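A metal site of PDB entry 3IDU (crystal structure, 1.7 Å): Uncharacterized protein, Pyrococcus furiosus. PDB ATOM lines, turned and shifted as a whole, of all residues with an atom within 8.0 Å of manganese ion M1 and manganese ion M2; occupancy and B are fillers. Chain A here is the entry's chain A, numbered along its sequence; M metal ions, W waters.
Manganese ion M1 is bound by OE2 of Glu 104 (2.2 Å), OD2 of Asp 97 (2.3 Å), OE2 of Glu 107 (2.3 Å), water W1 (2.3 Å), O of Val 102 (2.3 Å) and OD1 of Asn 100 (2.5 Å). Manganese ion M1 has six donor atoms within binding distance.
Water W1 lies within hydrogen-bond range of the backbone carbonyl oxygen (O) of Asp 97 (2.7 Å) and the side-chain amide nitrogen (ND2) of Asn 110 (3.4 Å).
The nearest printed residue that does not touch manganese ion M1 is Asn 110 (4.1 Å).
The backbone carbonyl oxygen (O) of Asp 18 lies within hydrogen-bond range of the backbone NH (N) of Leu 44 (2.8 Å). OD1 of Asp 97 lies within hydrogen-bond range of N of Thr 101. The backbone NH (N) of Asp 97 lies close to the side-chain hydroxyl (OG1) of Thr 52, at 3.5 Å. The backbone NH of Asp 18 is in hydrogen-bond range of the side-chain amide oxygen of Asn 43. O of Val 96 lies within hydrogen-bond range of ND2 of Asn 110. The backbone NH (N) of Asn 108 sits at hydrogen-bond distance from the side-chain amide oxygen (OD1) of Asn 106. The side-chain hydroxyl (OG1) of Thr 20 is in hydrogen-bond range of the backbone carbonyl oxygen (O) of Asn 109 (3.0 Å).
Manganese ion M2 is bound by OD1 of Asn 109 (2.2 Å), OD1 of Asn 110 (2.2 Å), O of Asn 106 (2.2 Å), OE1 of Glu 104 (2.2 Å), O of Leu 19 (2.2 Å) and OD1 of Asp 18 (2.3 Å).
Within 4 Å of manganese ion M2: Asp 18, Leu 19, Glu 104, Asn 106, Asn 109 and Asn 110.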
ATOM      1  N   PRO A  17      -3.238  20.720 -15.078  1.00  0.00           N
ATOM      2  CA  PRO A  17      -2.115  19.788 -15.104  1.00  0.00           C
ATOM      3  C   PRO A  17      -1.580  19.878 -16.532  1.00  0.00           C
ATOM      4  O   PRO A  17      -2.160  20.566 -17.368  1.00  0.00           O
ATOM      5  CB  PRO A  17      -2.784  18.433 -14.827  1.00  0.00           C
ATOM      6  CG  PRO A  17      -4.141  18.578 -15.449  1.00  0.00           C
ATOM      7  CD  PRO A  17      -4.531  20.010 -15.083  1.00  0.00           C
ATOM      8  N   ASP A  18      -0.446  19.241 -16.797  1.00  0.00           N
ATOM      9  CA  ASP A  18       0.087  19.196 -18.155  1.00  0.00           C
ATOM     10  C   ASP A  18       0.956  17.962 -18.270  1.00  0.00           C
ATOM     11  O   ASP A  18       2.087  17.922 -17.795  1.00  0.00           O
ATOM     12  CB  ASP A  18       0.916  20.420 -18.566  1.00  0.00           C
ATOM     13  CG  ASP A  18       1.319  20.365 -20.032  1.00  0.00           C
ATOM     14  OD1 ASP A  18       0.859  19.436 -20.726  1.00  0.00           O
ATOM     15  OD2 ASP A  18       2.078  21.238 -20.514  1.00  0.00           O
ATOM     16  N   LEU A  19       0.381  16.954 -18.891  1.00  0.00           N
ATOM     17  CA  LEU A  19       1.062  15.692 -19.077  1.00  0.00           C
ATOM     18  C   LEU A  19       1.989  15.715 -20.271  1.00  0.00           C
ATOM     19  O   LEU A  19       1.652  16.263 -21.318  1.00  0.00           O
ATOM     20  CB  LEU A  19       0.013  14.598 -19.268  1.00  0.00           C
ATOM     21  CG  LEU A  19      -0.940  14.454 -18.083  1.00  0.00           C
ATOM     22  CD1 LEU A  19      -2.174  13.659 -18.487  1.00  0.00           C
ATOM     23  CD2 LEU A  19      -0.206  13.761 -16.941  1.00  0.00           C
ATOM     24  N   THR A  20       3.157  15.104 -20.126  1.00  0.00           N
ATOM     25  CA  THR A  20       4.113  15.036 -21.217  1.00  0.00           C
ATOM     26  C   THR A  20       4.821  13.690 -21.145  1.00  0.00           C
ATOM     27  O   THR A  20       4.850  13.050 -20.083  1.00  0.00           O
ATOM     28  CB  THR A  20       5.154  16.168 -21.113  1.00  0.00           C
ATOM     29  OG1 THR A  20       5.824  16.301 -22.378  1.00  0.00           O
ATOM     30  CG2 THR A  20       6.177  15.857 -20.048  1.00  0.00           C
ATOM     31  N   VAL A  21       5.403  13.262 -22.259  1.00  0.00           N
ATOM     32  CA  VAL A  21       6.115  11.998 -22.304  1.00  0.00           C
ATOM     33  C   VAL A  21       7.393  12.096 -23.129  1.00  0.00           C
ATOM     34  O   VAL A  21       7.479  12.874 -24.075  1.00  0.00           O
ATOM     35  CB  VAL A  21       5.248  10.865 -22.916  1.00  0.00           C
ATOM     36  CG1 VAL A  21       4.105  10.511 -21.979  1.00  0.00           C
ATOM     37  CG2 VAL A  21       4.721  11.302 -24.271  1.00  0.00           C
ATOM     38  N   LYS A  42       5.666  13.076 -17.174  1.00  0.00           N
ATOM     39  CA  LYS A  42       5.685  14.157 -16.208  1.00  0.00           C
ATOM     40  C   LYS A  42       4.402  14.976 -16.200  1.00  0.00           C
ATOM     41  O   LYS A  42       3.673  15.004 -17.193  1.00  0.00           O
ATOM     42  CB  LYS A  42       6.859  15.096 -16.504  1.00  0.00           C
ATOM     43  CG  LYS A  42       8.148  14.351 -16.840  1.00  0.00           C
ATOM     44  CD  LYS A  42       9.239  15.253 -17.398  1.00  0.00           C
ATOM     45  CE  LYS A  42       9.886  16.109 -16.316  1.00  0.00           C
ATOM     46  NZ  LYS A  42      11.099  16.815 -16.829  1.00  0.00           N
ATOM     47  N   ASN A  43       4.134  15.614 -15.077  1.00  0.00           N
ATOM     48  CA  ASN A  43       2.989  16.503 -14.950  1.00  0.00           C
ATOM     49  C   ASN A  43       3.630  17.842 -14.640  1.00  0.00           C
ATOM     50  O   ASN A  43       4.091  18.068 -13.519  1.00  0.00           O
ATOM     51  CB  ASN A  43       2.077  16.113 -13.790  1.00  0.00           C
ATOM     52  CG  ASN A  43       0.908  17.070 -13.624  1.00  0.00           C
ATOM     53  OD1 ASN A  43       0.739  17.989 -14.423  1.00  0.00           O
ATOM     54  ND2 ASN A  43       0.096  16.839 -12.597  1.00  0.00           N
ATOM     55  N   LEU A  44       3.684  18.719 -15.639  1.00  0.00           N
ATOM     56  CA  LEU A  44       4.301  20.027 -15.462  1.00  0.00           C
ATOM     57  C   LEU A  44       3.371  21.008 -14.750  1.00  0.00           C
ATOM     58  O   LEU A  44       3.810  22.086 -14.338  1.00  0.00           O
ATOM     59  CB  LEU A  44       4.683  20.609 -16.814  1.00  0.00           C
ATOM     60  CG  LEU A  44       5.469  19.688 -17.757  1.00  0.00           C
ATOM     61  CD1 LEU A  44       5.647  20.366 -19.107  1.00  0.00           C
ATOM     62  CD2 LEU A  44       6.806  19.343 -17.133  1.00  0.00           C
ATOM     63  N   THR A  52      -4.376   8.350 -15.481  1.00  0.00           N
ATOM     64  CA  THR A  52      -4.285   8.564 -16.919  1.00  0.00           C
ATOM     65  C   THR A  52      -3.549   7.388 -17.526  1.00  0.00           C
ATOM     66  O   THR A  52      -2.792   6.687 -16.843  1.00  0.00           O
ATOM     67  CB  THR A  52      -3.556   9.877 -17.300  1.00  0.00           C
ATOM     68  OG1 THR A  52      -3.727  10.125 -18.699  1.00  0.00           O
ATOM     69  CG2 THR A  52      -2.077   9.785 -16.989  1.00  0.00           C
ATOM     70  N   VAL A  96       0.417   9.795 -23.758  1.00  0.00           N
ATOM     71  CA  VAL A  96      -0.192   9.909 -22.446  1.00  0.00           C
ATOM     72  C   VAL A  96      -1.517  10.636 -22.661  1.00  0.00           C
ATOM     73  O   VAL A  96      -1.602  11.596 -23.425  1.00  0.00           O
ATOM     74  CB  VAL A  96       0.737  10.639 -21.433  1.00  0.00           C
ATOM     75  CG1 VAL A  96       1.059  12.043 -21.929  1.00  0.00           C
ATOM     76  CG2 VAL A  96       0.073  10.678 -20.069  1.00  0.00           C
ATOM     77  N   ASP A  97      -2.561  10.146 -21.986  1.00  0.00           N
ATOM     78  CA  ASP A  97      -3.916  10.675 -22.130  1.00  0.00           C
ATOM     79  C   ASP A  97      -4.292  10.777 -23.596  1.00  0.00           C
ATOM     80  O   ASP A  97      -4.800  11.800 -24.049  1.00  0.00           O
ATOM     81  CB  ASP A  97      -4.088  12.035 -21.475  1.00  0.00           C
ATOM     82  CG  ASP A  97      -5.548  12.478 -21.460  1.00  0.00           C
ATOM     83  OD1 ASP A  97      -6.414  11.579 -21.375  1.00  0.00           O
ATOM     84  OD2 ASP A  97      -5.831  13.695 -21.537  1.00  0.00           O
ATOM     85  N   GLU A  98      -4.048   9.710 -24.340  1.00  0.00           N
ATOM     86  CA  GLU A  98      -4.372   9.708 -25.760  1.00  0.00           C
ATOM     87  C   GLU A  98      -5.863   9.909 -25.997  1.00  0.00           C
ATOM     88  O   GLU A  98      -6.253  10.468 -27.023  1.00  0.00           O
ATOM     89  CB  GLU A  98      -3.914   8.395 -26.385  1.00  0.00           C
ATOM     90  CG  GLU A  98      -3.645   8.492 -27.865  1.00  0.00           C
ATOM     91  CD  GLU A  98      -3.217   7.173 -28.462  1.00  0.00           C
ATOM     92  OE1 GLU A  98      -2.390   6.477 -27.829  1.00  0.00           O
ATOM     93  OE2 GLU A  98      -3.696   6.836 -29.557  1.00  0.00           O
ATOM     94  N   GLU A  99      -6.691   9.461 -25.066  1.00  0.00           N
ATOM     95  CA  GLU A  99      -8.150   9.601 -25.187  1.00  0.00           C
ATOM     96  C   GLU A  99      -8.594  10.995 -24.764  1.00  0.00           C
ATOM     97  O   GLU A  99      -9.784  11.318 -24.783  1.00  0.00           O
ATOM     98  CB  GLU A  99      -8.866   8.566 -24.316  1.00  0.00           C
ATOM     99  CG  GLU A  99      -8.370   8.524 -22.872  1.00  0.00           C
ATOM    100  CD  GLU A  99      -7.260   7.506 -22.674  1.00  0.00           C
ATOM    101  OE1 GLU A  99      -7.560   6.292 -22.732  1.00  0.00           O
ATOM    102  OE2 GLU A  99      -6.100   7.915 -22.467  1.00  0.00           O
ATOM    103  N   ASN A 100      -7.621  11.813 -24.399  1.00  0.00           N
ATOM    104  CA  ASN A 100      -7.823  13.180 -23.950  1.00  0.00           C
ATOM    105  C   ASN A 100      -9.004  13.346 -23.000  1.00  0.00           C
ATOM    106  O   ASN A 100     -10.007  13.998 -23.315  1.00  0.00           O
ATOM    107  CB  ASN A 100      -7.958  14.132 -25.132  1.00  0.00           C
ATOM    108  CG  ASN A 100      -7.984  15.584 -24.706  1.00  0.00           C
ATOM    109  OD1 ASN A 100      -7.332  15.974 -23.718  1.00  0.00           O
ATOM    110  ND2 ASN A 100      -8.725  16.402 -25.450  1.00  0.00           N
ATOM    111  N   THR A 101      -8.872  12.747 -21.826  1.00  0.00           N
ATOM    112  CA  THR A 101      -9.894  12.841 -20.794  1.00  0.00           C
ATOM    113  C   THR A 101      -9.421  13.799 -19.698  1.00  0.00           C
ATOM    114  O   THR A 101     -10.120  14.009 -18.702  1.00  0.00           O
ATOM    115  CB  THR A 101     -10.187  11.442 -20.192  1.00  0.00           C
ATOM    116  OG1 THR A 101      -8.961  10.849 -19.743  1.00  0.00           O
ATOM    117  CG2 THR A 101     -10.825  10.539 -21.236  1.00  0.00           C
ATOM    118  N   VAL A 102      -8.242  14.367 -19.893  1.00  0.00           N
ATOM    119  CA  VAL A 102      -7.665  15.319 -18.930  1.00  0.00           C
ATOM    120  C   VAL A 102      -7.402  16.666 -19.600  1.00  0.00           C
ATOM    121  O   VAL A 102      -6.649  16.736 -20.558  1.00  0.00           O
ATOM    122  CB  VAL A 102      -6.332  14.797 -18.355  1.00  0.00           C
ATOM    123  CG1 VAL A 102      -5.800  15.764 -17.315  1.00  0.00           C
ATOM    124  CG2 VAL A 102      -6.514  13.406 -17.752  1.00  0.00           C
ATOM    125  N   VAL A 103      -8.041  17.719 -19.107  1.00  0.00           N
ATOM    126  CA  VAL A 103      -7.828  19.061 -19.665  1.00  0.00           C
ATOM    127  C   VAL A 103      -6.490  19.549 -19.162  1.00  0.00           C
ATOM    128  O   VAL A 103      -6.281  19.662 -17.961  1.00  0.00           O
ATOM    129  CB  VAL A 103      -8.942  20.042 -19.231  1.00  0.00           C
ATOM    130  CG1 VAL A 103      -8.613  21.463 -19.699  1.00  0.00           C
ATOM    131  CG2 VAL A 103     -10.277  19.593 -19.835  1.00  0.00           C
ATOM    132  N   GLU A 104      -5.582  19.855 -20.085  1.00  0.00           N
ATOM    133  CA  GLU A 104      -4.237  20.310 -19.722  1.00  0.00           C
ATOM    134  C   GLU A 104      -3.868  21.638 -20.348  1.00  0.00           C
ATOM    135  O   GLU A 104      -4.580  22.175 -21.200  1.00  0.00           O
ATOM    136  CB  GLU A 104      -3.180  19.308 -20.191  1.00  0.00           C
ATOM    137  CG  GLU A 104      -3.430  17.855 -19.849  1.00  0.00           C
ATOM    138  CD  GLU A 104      -2.684  16.926 -20.806  1.00  0.00           C
ATOM    139  OE1 GLU A 104      -1.484  17.150 -21.043  1.00  0.00           O
ATOM    140  OE2 GLU A 104      -3.305  15.985 -21.331  1.00  0.00           O
ATOM    141  N   LEU A 105      -2.717  22.141 -19.933  1.00  0.00           N
ATOM    142  CA  LEU A 105      -2.178  23.387 -20.447  1.00  0.00           C
ATOM    143  C   LEU A 105      -1.778  23.194 -21.914  1.00  0.00           C
ATOM    144  O   LEU A 105      -1.737  24.136 -22.690  1.00  0.00           O
ATOM    145  CB  LEU A 105      -0.948  23.801 -19.652  1.00  0.00           C
ATOM    146  CG  LEU A 105      -1.102  23.988 -18.154  1.00  0.00           C
ATOM    147  CD1 LEU A 105       0.267  24.128 -17.508  1.00  0.00           C
ATOM    148  CD2 LEU A 105      -1.961  25.218 -17.869  1.00  0.00           C
ATOM    149  N   ASN A 106      -1.478  21.953 -22.282  1.00  0.00           N
ATOM    150  CA  ASN A 106      -1.053  21.640 -23.644  1.00  0.00           C
ATOM    151  C   ASN A 106      -1.406  20.193 -23.968  1.00  0.00           C
ATOM    152  O   ASN A 106      -1.074  19.277 -23.211  1.00  0.00           O
ATOM    153  CB  ASN A 106       0.464  21.862 -23.765  1.00  0.00           C
ATOM    154  CG  ASN A 106       0.977  21.717 -25.183  1.00  0.00           C
ATOM    155  OD1 ASN A 106       0.248  21.351 -26.095  1.00  0.00           O
ATOM    156  ND2 ASN A 106       2.264  22.012 -25.372  1.00  0.00           N
ATOM    157  N   GLU A 107      -2.117  19.988 -25.079  1.00  0.00           N
ATOM    158  CA  GLU A 107      -2.498  18.633 -25.478  1.00  0.00           C
ATOM    159  C   GLU A 107      -1.596  18.183 -26.631  1.00  0.00           C
ATOM    160  O   GLU A 107      -1.707  17.053 -27.121  1.00  0.00           O
ATOM    161  CB  GLU A 107      -3.970  18.595 -25.945  1.00  0.00           C
ATOM    162  CG  GLU A 107      -4.960  19.369 -25.069  1.00  0.00           C
ATOM    163  CD  GLU A 107      -5.163  18.760 -23.693  1.00  0.00           C
ATOM    164  OE1 GLU A 107      -5.851  19.407 -22.851  1.00  0.00           O
ATOM    165  OE2 GLU A 107      -4.656  17.641 -23.434  1.00  0.00           O
ATOM    166  N   ASN A 108      -0.696  19.066 -27.048  1.00  0.00           N
ATOM    167  CA  ASN A 108       0.188  18.758 -28.165  1.00  0.00           C
ATOM    168  C   ASN A 108       1.599  18.303 -27.776  1.00  0.00           C
ATOM    169  O   ASN A 108       2.466  18.169 -28.638  1.00  0.00           O
ATOM    170  CB  ASN A 108       0.254  19.973 -29.108  1.00  0.00           C
ATOM    171  CG  ASN A 108      -1.128  20.432 -29.553  1.00  0.00           C
ATOM    172  OD1 ASN A 108      -1.621  21.478 -29.108  1.00  0.00           O
ATOM    173  ND2 ASN A 108      -1.758  19.641 -30.418  1.00  0.00           N
ATOM    174  N   ASN A 109       1.821  18.060 -26.489  1.00  0.00           N
ATOM    175  CA  ASN A 109       3.125  17.578 -26.022  1.00  0.00           C
ATOM    176  C   ASN A 109       2.901  16.240 -25.323  1.00  0.00           C
ATOM    177  O   ASN A 109       3.678  15.834 -24.448  1.00  0.00           O
ATOM    178  CB  ASN A 109       3.771  18.587 -25.061  1.00  0.00           C
ATOM    179  CG  ASN A 109       2.926  18.858 -23.821  1.00  0.00           C
ATOM    180  OD1 ASN A 109       1.781  18.422 -23.730  1.00  0.00           O
ATOM    181  ND2 ASN A 109       3.487  19.589 -22.863  1.00  0.00           N
ATOM    182  N   ASN A 110       1.838  15.561 -25.723  1.00  0.00           N
ATOM    183  CA  ASN A 110       1.470  14.274 -25.141  1.00  0.00           C
ATOM    184  C   ASN A 110       1.955  13.081 -25.948  1.00  0.00           C
ATOM    185  O   ASN A 110       1.587  11.948 -25.649  1.00  0.00           O
ATOM    186  CB  ASN A 110      -0.046  14.198 -24.985  1.00  0.00           C
ATOM    187  CG  ASN A 110      -0.574  15.106 -23.897  1.00  0.00           C
ATOM    188  OD1 ASN A 110      -0.214  16.276 -23.823  1.00  0.00           O
ATOM    189  ND2 ASN A 110      -1.436  14.575 -23.048  1.00  0.00           N
ATOM    190  N   VAL A 111       2.764  13.325 -26.976  1.00  0.00           N
ATOM    191  CA  VAL A 111       3.266  12.243 -27.809  1.00  0.00           C
ATOM    192  C   VAL A 111       4.773  12.315 -28.008  1.00  0.00           C
ATOM    193  O   VAL A 111       5.320  13.376 -28.324  1.00  0.00           O
ATOM    194  CB  VAL A 111       2.592  12.257 -29.190  1.00  0.00           C
ATOM    195  CG1 VAL A 111       3.134  11.131 -30.056  1.00  0.00           C
ATOM    196  CG2 VAL A 111       1.077  12.123 -29.045  1.00  0.00           C
HETATM  197 MN    MN M   1      -5.302  15.776 -22.222  1.00  0.00          MN
HETATM  198 MN    MN M   2       0.289  17.773 -22.275  1.00  0.00          MN
HETATM  199  O   HOH W   1      -4.650  14.470 -24.041  1.00  0.00           O
